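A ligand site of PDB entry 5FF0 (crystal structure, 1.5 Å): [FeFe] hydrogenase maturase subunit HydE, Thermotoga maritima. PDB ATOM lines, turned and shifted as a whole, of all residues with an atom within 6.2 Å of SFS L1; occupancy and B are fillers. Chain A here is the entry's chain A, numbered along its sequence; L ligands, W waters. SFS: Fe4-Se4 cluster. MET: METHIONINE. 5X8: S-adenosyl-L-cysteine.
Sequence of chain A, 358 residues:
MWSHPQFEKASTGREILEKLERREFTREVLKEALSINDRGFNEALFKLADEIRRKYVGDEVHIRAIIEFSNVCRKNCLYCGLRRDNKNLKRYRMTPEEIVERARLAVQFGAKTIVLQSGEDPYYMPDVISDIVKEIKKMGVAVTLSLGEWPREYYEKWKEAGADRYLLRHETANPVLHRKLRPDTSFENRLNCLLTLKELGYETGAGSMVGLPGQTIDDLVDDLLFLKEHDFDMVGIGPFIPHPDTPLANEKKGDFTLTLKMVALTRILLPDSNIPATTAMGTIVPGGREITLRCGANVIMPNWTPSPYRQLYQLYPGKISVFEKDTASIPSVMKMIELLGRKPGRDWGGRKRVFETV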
ATOM      1  N   VAL A  72      21.105  -7.749 -29.286  1.00  0.00           N
ATOM      2  CA  VAL A  72      22.298  -7.899 -30.158  1.00  0.00           C
ATOM      3  C   VAL A  72      23.535  -7.735 -29.317  1.00  0.00           C
ATOM      4  O   VAL A  72      23.654  -6.761 -28.580  1.00  0.00           O
ATOM      5  CB  VAL A  72      22.255  -6.926 -31.314  1.00  0.00           C
ATOM      6  CG1 VAL A  72      23.572  -6.969 -32.111  1.00  0.00           C
ATOM      7  CG2 VAL A  72      21.039  -7.193 -32.197  1.00  0.00           C
ATOM      8  N   CYS A  73      24.509  -8.633 -29.424  1.00  0.00           N
ATOM      9  CA  CYS A  73      25.779  -8.469 -28.753  1.00  0.00           C
ATOM     10  C   CYS A  73      26.957  -8.914 -29.590  1.00  0.00           C
ATOM     11  O   CYS A  73      26.893  -9.928 -30.239  1.00  0.00           O
ATOM     12  CB  CYS A  73      25.838  -9.236 -27.404  1.00  0.00           C
ATOM     13  SG  CYS A  73      27.179  -8.662 -26.335  1.00  0.00           S
ATOM     14  N   ARG A  74      28.001  -8.110 -29.542  1.00  0.00           N
ATOM     15  CA  ARG A  74      29.287  -8.404 -30.216  1.00  0.00           C
ATOM     16  C   ARG A  74      30.182  -9.295 -29.400  1.00  0.00           C
ATOM     17  O   ARG A  74      31.179  -9.813 -29.963  1.00  0.00           O
ATOM     18  CB  ARG A  74      30.006  -7.103 -30.541  1.00  0.00           C
ATOM     19  CG  ARG A  74      30.533  -6.380 -29.312  1.00  0.00           C
ATOM     20  CD  ARG A  74      31.102  -5.047 -29.628  1.00  0.00           C
ATOM     21  NE  ARG A  74      31.497  -4.334 -28.446  1.00  0.00           N
ATOM     22  CZ  ARG A  74      32.280  -3.302 -28.422  1.00  0.00           C
ATOM     23  NH1 ARG A  74      32.812  -2.801 -29.530  1.00  0.00           N
ATOM     24  NH2 ARG A  74      32.596  -2.738 -27.262  1.00  0.00           N
ATOM     25  N   LYS A  75      29.959  -9.498 -28.126  1.00  0.00           N
ATOM     26  CA  LYS A  75      30.800 -10.304 -27.237  1.00  0.00           C
ATOM     27  C   LYS A  75      30.278 -11.721 -27.141  1.00  0.00           C
ATOM     28  O   LYS A  75      29.186 -12.042 -27.618  1.00  0.00           O
ATOM     29  CB  LYS A  75      30.985  -9.644 -25.886  1.00  0.00           C
ATOM     30  CG  LYS A  75      31.993  -8.495 -25.873  1.00  0.00           C
ATOM     31  CD  LYS A  75      32.282  -7.968 -24.528  1.00  0.00           C
ATOM     32  CE  LYS A  75      33.483  -7.060 -24.405  1.00  0.00           C
ATOM     33  NZ  LYS A  75      33.509  -5.943 -25.373  1.00  0.00           N
ATOM     34  N   ASN A  76      31.080 -12.588 -26.497  1.00  0.00           N
ATOM     35  CA  ASN A  76      30.858 -14.023 -26.525  1.00  0.00           C
ATOM     36  C   ASN A  76      31.036 -14.635 -25.146  1.00  0.00           C
ATOM     37  O   ASN A  76      31.511 -15.778 -25.008  1.00  0.00           O
ATOM     38  CB  ASN A  76      31.775 -14.692 -27.512  1.00  0.00           C
ATOM     39  CG  ASN A  76      31.186 -15.907 -28.164  1.00  0.00           C
ATOM     40  OD1 ASN A  76      30.024 -16.102 -28.310  1.00  0.00           O
ATOM     41  ND2 ASN A  76      32.116 -16.780 -28.697  1.00  0.00           N
ATOM     42  N   CYS A  77      30.637 -13.904 -24.103  1.00  0.00           N
ATOM     43  CA  CYS A  77      30.797 -14.398 -22.730  1.00  0.00           C
ATOM     44  C   CYS A  77      30.213 -15.798 -22.604  1.00  0.00           C
ATOM     45  O   CYS A  77      29.129 -16.083 -23.070  1.00  0.00           O
ATOM     46  CB  CYS A  77      30.109 -13.409 -21.722  1.00  0.00           C
ATOM     47  SG  CYS A  77      30.666 -11.710 -21.918  1.00  0.00           S
ATOM     48  N   TYR A  79      29.011 -17.570 -20.319  1.00  0.00           N
ATOM     49  CA  TYR A  79      27.833 -17.817 -19.444  1.00  0.00           C
ATOM     50  C   TYR A  79      26.525 -17.294 -20.029  1.00  0.00           C
ATOM     51  O   TYR A  79      25.469 -17.656 -19.618  1.00  0.00           O
ATOM     52  CB  TYR A  79      28.059 -17.204 -18.062  1.00  0.00           C
ATOM     53  CG  TYR A  79      28.646 -15.804 -18.064  1.00  0.00           C
ATOM     54  CD1 TYR A  79      27.831 -14.682 -18.320  1.00  0.00           C
ATOM     55  CD2 TYR A  79      30.000 -15.580 -17.826  1.00  0.00           C
ATOM     56  CE1 TYR A  79      28.369 -13.398 -18.337  1.00  0.00           C
ATOM     57  CE2 TYR A  79      30.525 -14.294 -17.869  1.00  0.00           C
ATOM     58  CZ  TYR A  79      29.702 -13.214 -18.100  1.00  0.00           C
ATOM     59  OH  TYR A  79      30.280 -12.034 -18.153  1.00  0.00           O
ATOM     60  N   CYS A  80      26.598 -16.338 -20.953  1.00  0.00           N
ATOM     61  CA  CYS A  80      25.433 -15.562 -21.348  1.00  0.00           C
ATOM     62  C   CYS A  80      24.622 -16.061 -22.529  1.00  0.00           C
ATOM     63  O   CYS A  80      25.194 -16.308 -23.531  1.00  0.00           O
ATOM     64  CB  CYS A  80      25.932 -14.180 -21.672  1.00  0.00           C
ATOM     65  SG  CYS A  80      24.595 -12.974 -21.999  1.00  0.00           S
ATOM     66  N   GLY A  81      23.295 -16.121 -22.444  1.00  0.00           N
ATOM     67  CA  GLY A  81      22.457 -16.477 -23.533  1.00  0.00           C
ATOM     68  C   GLY A  81      22.424 -15.572 -24.727  1.00  0.00           C
ATOM     69  O   GLY A  81      21.936 -15.965 -25.796  1.00  0.00           O
ATOM     70  N   LEU A  82      22.899 -14.329 -24.579  1.00  0.00           N
ATOM     71  CA  LEU A  82      22.987 -13.408 -25.686  1.00  0.00           C
ATOM     72  C   LEU A  82      24.329 -13.434 -26.426  1.00  0.00           C
ATOM     73  O   LEU A  82      24.501 -12.703 -27.377  1.00  0.00           O
ATOM     74  CB  LEU A  82      22.690 -11.962 -25.240  1.00  0.00           C
ATOM     75  CG  LEU A  82      21.387 -11.733 -24.546  1.00  0.00           C
ATOM     76  CD1 LEU A  82      21.178 -10.224 -24.344  1.00  0.00           C
ATOM     77  CD2 LEU A  82      20.199 -12.408 -25.002  1.00  0.00           C
ATOM     78  N   ARG A  83      25.226 -14.310 -26.018  1.00  0.00           N
ATOM     79  CA  ARG A  83      26.537 -14.373 -26.664  1.00  0.00           C
ATOM     80  C   ARG A  83      26.412 -14.487 -28.144  1.00  0.00           C
ATOM     81  O   ARG A  83      25.536 -15.116 -28.690  1.00  0.00           O
ATOM     82  CB  ARG A  83      27.368 -15.523 -26.056  1.00  0.00           C
ATOM     83  CG  ARG A  83      26.813 -16.918 -26.359  1.00  0.00           C
ATOM     84  CD  ARG A  83      27.416 -17.931 -25.418  1.00  0.00           C
ATOM     85  NE  ARG A  83      28.856 -17.879 -25.364  1.00  0.00           N
ATOM     86  CZ  ARG A  83      29.702 -18.578 -26.159  1.00  0.00           C
ATOM     87  NH1 ARG A  83      29.183 -19.417 -27.050  1.00  0.00           N
ATOM     88  NH2 ARG A  83      30.964 -18.403 -26.031  1.00  0.00           N
ATOM     89  N   ARG A  84      27.387 -13.880 -28.855  1.00  0.00           N
ATOM     90  CA  ARG A  84      27.282 -13.811 -30.323  1.00  0.00           C
ATOM     91  C   ARG A  84      27.205 -15.157 -31.012  1.00  0.00           C
ATOM     92  O   ARG A  84      26.565 -15.254 -32.053  1.00  0.00           O
ATOM     93  CB  ARG A  84      28.358 -12.981 -30.945  1.00  0.00           C
ATOM     94  CG  ARG A  84      29.717 -13.528 -30.860  1.00  0.00           C
ATOM     95  CD  ARG A  84      30.733 -12.702 -31.756  1.00  0.00           C
ATOM     96  NE  ARG A  84      31.986 -13.407 -31.642  1.00  0.00           N
ATOM     97  CZ  ARG A  84      32.920 -13.180 -30.763  1.00  0.00           C
ATOM     98  NH1 ARG A  84      32.872 -12.161 -29.927  1.00  0.00           N
ATOM     99  NH2 ARG A  84      33.920 -14.046 -30.651  1.00  0.00           N
ATOM    100  N   SER A 118      21.273  -3.329 -22.649  1.00  0.00           N
ATOM    101  CA  SER A 118      21.320  -4.048 -23.904  1.00  0.00           C
ATOM    102  C   SER A 118      22.526  -4.952 -23.916  1.00  0.00           C
ATOM    103  O   SER A 118      23.451  -4.838 -23.118  1.00  0.00           O
ATOM    104  CB  SER A 118      21.373  -3.069 -25.101  1.00  0.00           C
ATOM    105  OG  SER A 118      22.521  -2.254 -25.047  1.00  0.00           O
ATOM    106  N   GLY A 119      22.546  -5.836 -24.925  1.00  0.00           N
ATOM    107  CA  GLY A 119      23.812  -6.414 -25.382  1.00  0.00           C
ATOM    108  C   GLY A 119      24.736  -5.303 -25.838  1.00  0.00           C
ATOM    109  O   GLY A 119      24.322  -4.135 -26.034  1.00  0.00           O
ATOM    110  N   GLU A 120      26.007  -5.607 -26.032  1.00  0.00           N
ATOM    111  CA  GLU A 120      26.917  -4.659 -26.651  1.00  0.00           C
ATOM    112  C   GLU A 120      26.616  -4.548 -28.129  1.00  0.00           C
ATOM    113  O   GLU A 120      27.270  -5.231 -28.978  1.00  0.00           O
ATOM    114  CB  GLU A 120      28.370  -5.016 -26.388  1.00  0.00           C
ATOM    115  CG  GLU A 120      28.792  -4.825 -24.948  1.00  0.00           C
ATOM    116  CD  GLU A 120      30.285  -4.861 -24.732  1.00  0.00           C
ATOM    117  OE1 GLU A 120      31.036  -4.902 -25.726  1.00  0.00           O
ATOM    118  OE2 GLU A 120      30.726  -4.853 -23.561  1.00  0.00           O
ATOM    119  N   GLY A 148      27.534  -2.120 -21.269  1.00  0.00           N
ATOM    120  CA  GLY A 148      28.810  -2.819 -21.462  1.00  0.00           C
ATOM    121  C   GLY A 148      30.005  -1.890 -21.551  1.00  0.00           C
ATOM    122  O   GLY A 148      29.988  -0.757 -21.075  1.00  0.00           O
ATOM    123  N   GLU A 171      31.779  -8.918 -12.549  1.00  0.00           N
ATOM    124  CA  GLU A 171      31.544 -10.306 -12.901  1.00  0.00           C
ATOM    125  C   GLU A 171      32.320 -11.306 -12.012  1.00  0.00           C
ATOM    126  O   GLU A 171      31.718 -12.144 -11.364  1.00  0.00           O
ATOM    127  CB  GLU A 171      31.756 -10.607 -14.394  1.00  0.00           C
ATOM    128  CG  GLU A 171      31.047  -9.654 -15.334  1.00  0.00           C
ATOM    129  CD  GLU A 171      29.540  -9.600 -15.203  1.00  0.00           C
ATOM    130  OE1 GLU A 171      28.962 -10.241 -14.323  1.00  0.00           O
ATOM    131  OE2 GLU A 171      28.908  -8.897 -16.065  1.00  0.00           O
ATOM    132  N   ARG A 182      35.161 -14.461 -20.337  1.00  0.00           N
ATOM    133  CA  ARG A 182      34.862 -13.297 -21.167  1.00  0.00           C
ATOM    134  C   ARG A 182      36.051 -13.120 -22.112  1.00  0.00           C
ATOM    135  O   ARG A 182      36.881 -12.298 -21.913  1.00  0.00           O
ATOM    136  CB  ARG A 182      34.653 -12.087 -20.243  1.00  0.00           C
ATOM    137  CG  ARG A 182      33.687 -12.396 -19.077  1.00  0.00           C
ATOM    138  CD  ARG A 182      33.266 -11.151 -18.310  1.00  0.00           C
ATOM    139  NE  ARG A 182      32.497 -10.322 -19.197  1.00  0.00           N
ATOM    140  CZ  ARG A 182      32.873  -9.136 -19.605  1.00  0.00           C
ATOM    141  NH1 ARG A 182      33.909  -8.522 -19.104  1.00  0.00           N
ATOM    142  NH2 ARG A 182      32.129  -8.566 -20.550  1.00  0.00           N
ATOM    143  N   ARG A 190      37.736  -4.220 -17.701  1.00  0.00           N
ATOM    144  CA  ARG A 190      36.495  -3.996 -16.940  1.00  0.00           C
ATOM    145  C   ARG A 190      36.682  -2.991 -15.848  1.00  0.00           C
ATOM    146  O   ARG A 190      35.891  -2.053 -15.655  1.00  0.00           O
ATOM    147  CB  ARG A 190      36.040  -5.356 -16.354  1.00  0.00           C
ATOM    148  CG  ARG A 190      34.569  -5.418 -15.909  1.00  0.00           C
ATOM    149  CD  ARG A 190      33.685  -5.509 -17.140  1.00  0.00           C
ATOM    150  NE  ARG A 190      32.292  -5.840 -16.789  1.00  0.00           N
ATOM    151  CZ  ARG A 190      31.315  -5.908 -17.688  1.00  0.00           C
ATOM    152  NH1 ARG A 190      31.552  -5.699 -18.972  1.00  0.00           N
ATOM    153  NH2 ARG A 190      30.082  -6.130 -17.275  1.00  0.00           N
ATOM    154  N   TYR A 313      15.033 -11.768 -24.370  1.00  0.00           N
ATOM    155  CA  TYR A 313      16.158 -11.291 -23.620  1.00  0.00           C
ATOM    156  C   TYR A 313      16.308 -12.170 -22.401  1.00  0.00           C
ATOM    157  O   TYR A 313      15.858 -11.868 -21.350  1.00  0.00           O
ATOM    158  CB  TYR A 313      15.991  -9.824 -23.221  1.00  0.00           C
ATOM    159  CG  TYR A 313      17.237  -9.089 -22.815  1.00  0.00           C
ATOM    160  CD1 TYR A 313      17.884  -8.279 -23.706  1.00  0.00           C
ATOM    161  CD2 TYR A 313      17.730  -9.172 -21.580  1.00  0.00           C
ATOM    162  CE1 TYR A 313      18.992  -7.558 -23.360  1.00  0.00           C
ATOM    163  CE2 TYR A 313      18.821  -8.453 -21.215  1.00  0.00           C
ATOM    164  CZ  TYR A 313      19.455  -7.650 -22.131  1.00  0.00           C
ATOM    165  OH  TYR A 313      20.533  -6.927 -21.760  1.00  0.00           O
ATOM    166  N   LEU A 315      19.270 -13.878 -20.595  1.00  0.00           N
ATOM    167  CA  LEU A 315      20.669 -14.105 -20.288  1.00  0.00           C
ATOM    168  C   LEU A 315      20.803 -15.497 -19.677  1.00  0.00           C
ATOM    169  O   LEU A 315      21.771 -16.141 -19.852  1.00  0.00           O
ATOM    170  CB  LEU A 315      21.148 -13.084 -19.258  1.00  0.00           C
ATOM    171  CG  LEU A 315      20.811 -11.637 -19.518  1.00  0.00           C
ATOM    172  CD1 LEU A 315      21.368 -10.726 -18.409  1.00  0.00           C
ATOM    173  CD2 LEU A 315      21.287 -11.219 -20.788  1.00  0.00           C
HETATM  174 SE4  SFS L   1      27.577 -11.853 -24.107  1.00  0.00          SE
HETATM  175 FE1  SFS L   1      25.949 -11.180 -22.457  1.00  0.00          FE
HETATM  176 FE3  SFS L   1      28.599 -10.642 -22.291  1.00  0.00          FE
HETATM  177 FE2  SFS L   1      27.053  -9.581 -24.302  1.00  0.00          FE
HETATM  178 SE3  SFS L   1      24.949  -9.276 -23.257  1.00  0.00          SE
HETATM  179 FE4  SFS L   1      26.554  -8.520 -21.553  1.00  0.00          FE
HETATM  180 SE2  SFS L   1      27.113 -10.667 -20.390  1.00  0.00          SE
HETATM  181 SE1  SFS L   1      28.686  -8.404 -22.967  1.00  0.00          SE
HETATM  182  N   MET L   2      26.080  -6.283 -21.741  1.00  0.00           N
HETATM  183  CA  MET L   2      26.149  -5.428 -20.514  1.00  0.00           C
HETATM  184  C   MET L   2      27.237  -6.023 -19.666  1.00  0.00           C
HETATM  185  O   MET L   2      27.634  -5.376 -18.727  1.00  0.00           O
HETATM  186  CB  MET L   2      24.779  -5.424 -19.785  1.00  0.00           C
HETATM  187  CG  MET L   2      24.573  -6.627 -18.883  1.00  0.00           C
HETATM  188  SD  MET L   2      24.469  -8.241 -19.732  1.00  0.00           S
HETATM  189  CE  MET L   2      22.961  -7.841 -20.554  1.00  0.00           C
HETATM  190  OXT MET L   2      27.658  -7.215 -19.895  1.00  0.00           O
HETATM  191  N1  5X8 L   3      23.273 -16.323 -15.049  1.00  0.00           N
HETATM  192  C5  5X8 L   3      24.007 -14.802 -16.586  1.00  0.00           C
HETATM  193  C8  5X8 L   3      24.622 -12.901 -17.392  1.00  0.00           C
HETATM  194  C2  5X8 L   3      23.132 -15.344 -14.148  1.00  0.00           C
HETATM  195  C6  5X8 L   3      23.716 -16.048 -16.285  1.00  0.00           C
HETATM  196  N3  5X8 L   3      23.421 -14.109 -14.479  1.00  0.00           N
HETATM  197  C4  5X8 L   3      23.867 -13.835 -15.657  1.00  0.00           C
HETATM  198  O   5X8 L   3      18.319 -10.601 -14.353  1.00  0.00           O
HETATM  199  C   5X8 L   3      18.987 -10.128 -13.418  1.00  0.00           C
HETATM  200  OXT 5X8 L   3      19.271 -10.659 -12.406  1.00  0.00           O
HETATM  201  CA  5X8 L   3      19.713  -8.847 -13.767  1.00  0.00           C
HETATM  202  N   5X8 L   3      19.915  -8.124 -12.503  1.00  0.00           N
HETATM  203  CB  5X8 L   3      20.967  -9.142 -14.573  1.00  0.00           C
HETATM  204  SG  5X8 L   3      21.916  -7.570 -14.957  1.00  0.00           S
HETATM  205  C5' 5X8 L   3      23.361  -8.197 -16.088  1.00  0.00           C
HETATM  206  C4' 5X8 L   3      24.209  -9.213 -15.461  1.00  0.00           C
HETATM  207  O4' 5X8 L   3      23.553 -10.453 -15.633  1.00  0.00           O
HETATM  208  C3' 5X8 L   3      25.519  -9.440 -16.177  1.00  0.00           C
HETATM  209  O3' 5X8 L   3      26.424  -8.405 -15.770  1.00  0.00           O
HETATM  210  C2' 5X8 L   3      25.834 -10.813 -15.539  1.00  0.00           C
HETATM  211  O2' 5X8 L   3      26.401 -10.708 -14.199  1.00  0.00           O
HETATM  212  C1' 5X8 L   3      24.423 -11.465 -15.347  1.00  0.00           C
HETATM  213  N9  5X8 L   3      24.264 -12.676 -16.103  1.00  0.00           N
HETATM  214  N7  5X8 L   3      24.451 -14.187 -17.675  1.00  0.00           N
HETATM  215  N6  5X8 L   3      23.790 -17.034 -17.137  1.00  0.00           N
HETATM  216  O   HOH W   1      30.015  -5.992 -21.274  1.00  0.00           O
HETATM  217  O   HOH W   2      29.479  -9.332 -18.681  1.00  0.00           O
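An iron atom (FE2) of SFS L1 is bound by the side-chain sulfur of Cys 73. The backbone carbonyl oxygen (O) of Tyr 79 sits at hydrogen-bond distance from a nitrogen (N6) of 5X8 L3. The backbone carbonyl oxygen (O) of Leu 315 is in hydrogen-bond range of a nitrogen (N6) of 5X8 L3. The side-chain carboxylate (OE2) of Glu 171 is in hydrogen-bond range of an oxygen (O3') of 5X8 L3, 2.5 Å away. A nitrogen (N) of MET L2 lies close to the backbone carbonyl oxygen (O) of Ser 118, at 3.3 Å. An iron atom (FE1) of SFS L1 is bound by the side-chain sulfur (SG) of Cys 80 (2.3 Å). SG of Cys 77 is bound to FE3 of SFS L1 (2.4 Å). O of MET L2 lies within salt-bridge range of NH2 of Arg 190 (2.9 Å).
Water W2 lies within hydrogen-bond range of OE2 of Glu 171 (2.7 Å), OH of Tyr 79 (2.9 Å) and NE of Arg 182 (3.2 Å). Water W1 lies within hydrogen-bond range of OE2 of Glu 120 (2.7 Å), NH1 of Arg 190 (2.8 Å) and NH2 of Arg 182 (3.4 Å).
The side-chain hydroxyl of Tyr 79 lies within hydrogen-bond range of the guanidinium group of Arg 182 (3.0 Å). O of Lys 75 sits at hydrogen-bond distance from N of Arg 84 (2.9 Å). The guanidinium group of Arg 83 sits at hydrogen-bond distance from the backbone carbonyl oxygen of Cys 77, at 2.9 Å. The backbone NH of Glu 120 sits close to the side-chain sulfur of Cys 73, 3.3 Å away. The side-chain sulfur (SG) of Cys 80 sits close to the backbone NH (N) of Leu 82, 3.4 Å away. SG of Cys 77 lies close to NE of Arg 182 (3.6 Å). N of Lys 75 lies close to SG of Cys 73 (3.4 Å). The backbone carbonyl oxygen of Asn 76 lies within hydrogen-bond range of the guanidinium group of Arg 83.
Residues that only touch SFS L1: Tyr 79 (3.6 Å), Arg 83 (3.7 Å), Gly 119 (3.7 Å) and Lys 75 (3.9 Å). Hydrophobic or aromatic side chains that line SFS L1: Tyr 79. Seven residues have an atom within 4 Å of SFS L1: Cys 73, Lys 75, Cys 77, Tyr 79, Cys 80, Arg 83 and Gly 119. Along chain A the residues within 4 Å of SFS L1 span positions 73 to 119. The nearest printed residue that does not touch SFS L1 is Leu 82 (4.03 Å).
A nitrogen (N) of MET L2 binds an iron atom (FE4) of SFS L1 (2.3 Å).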
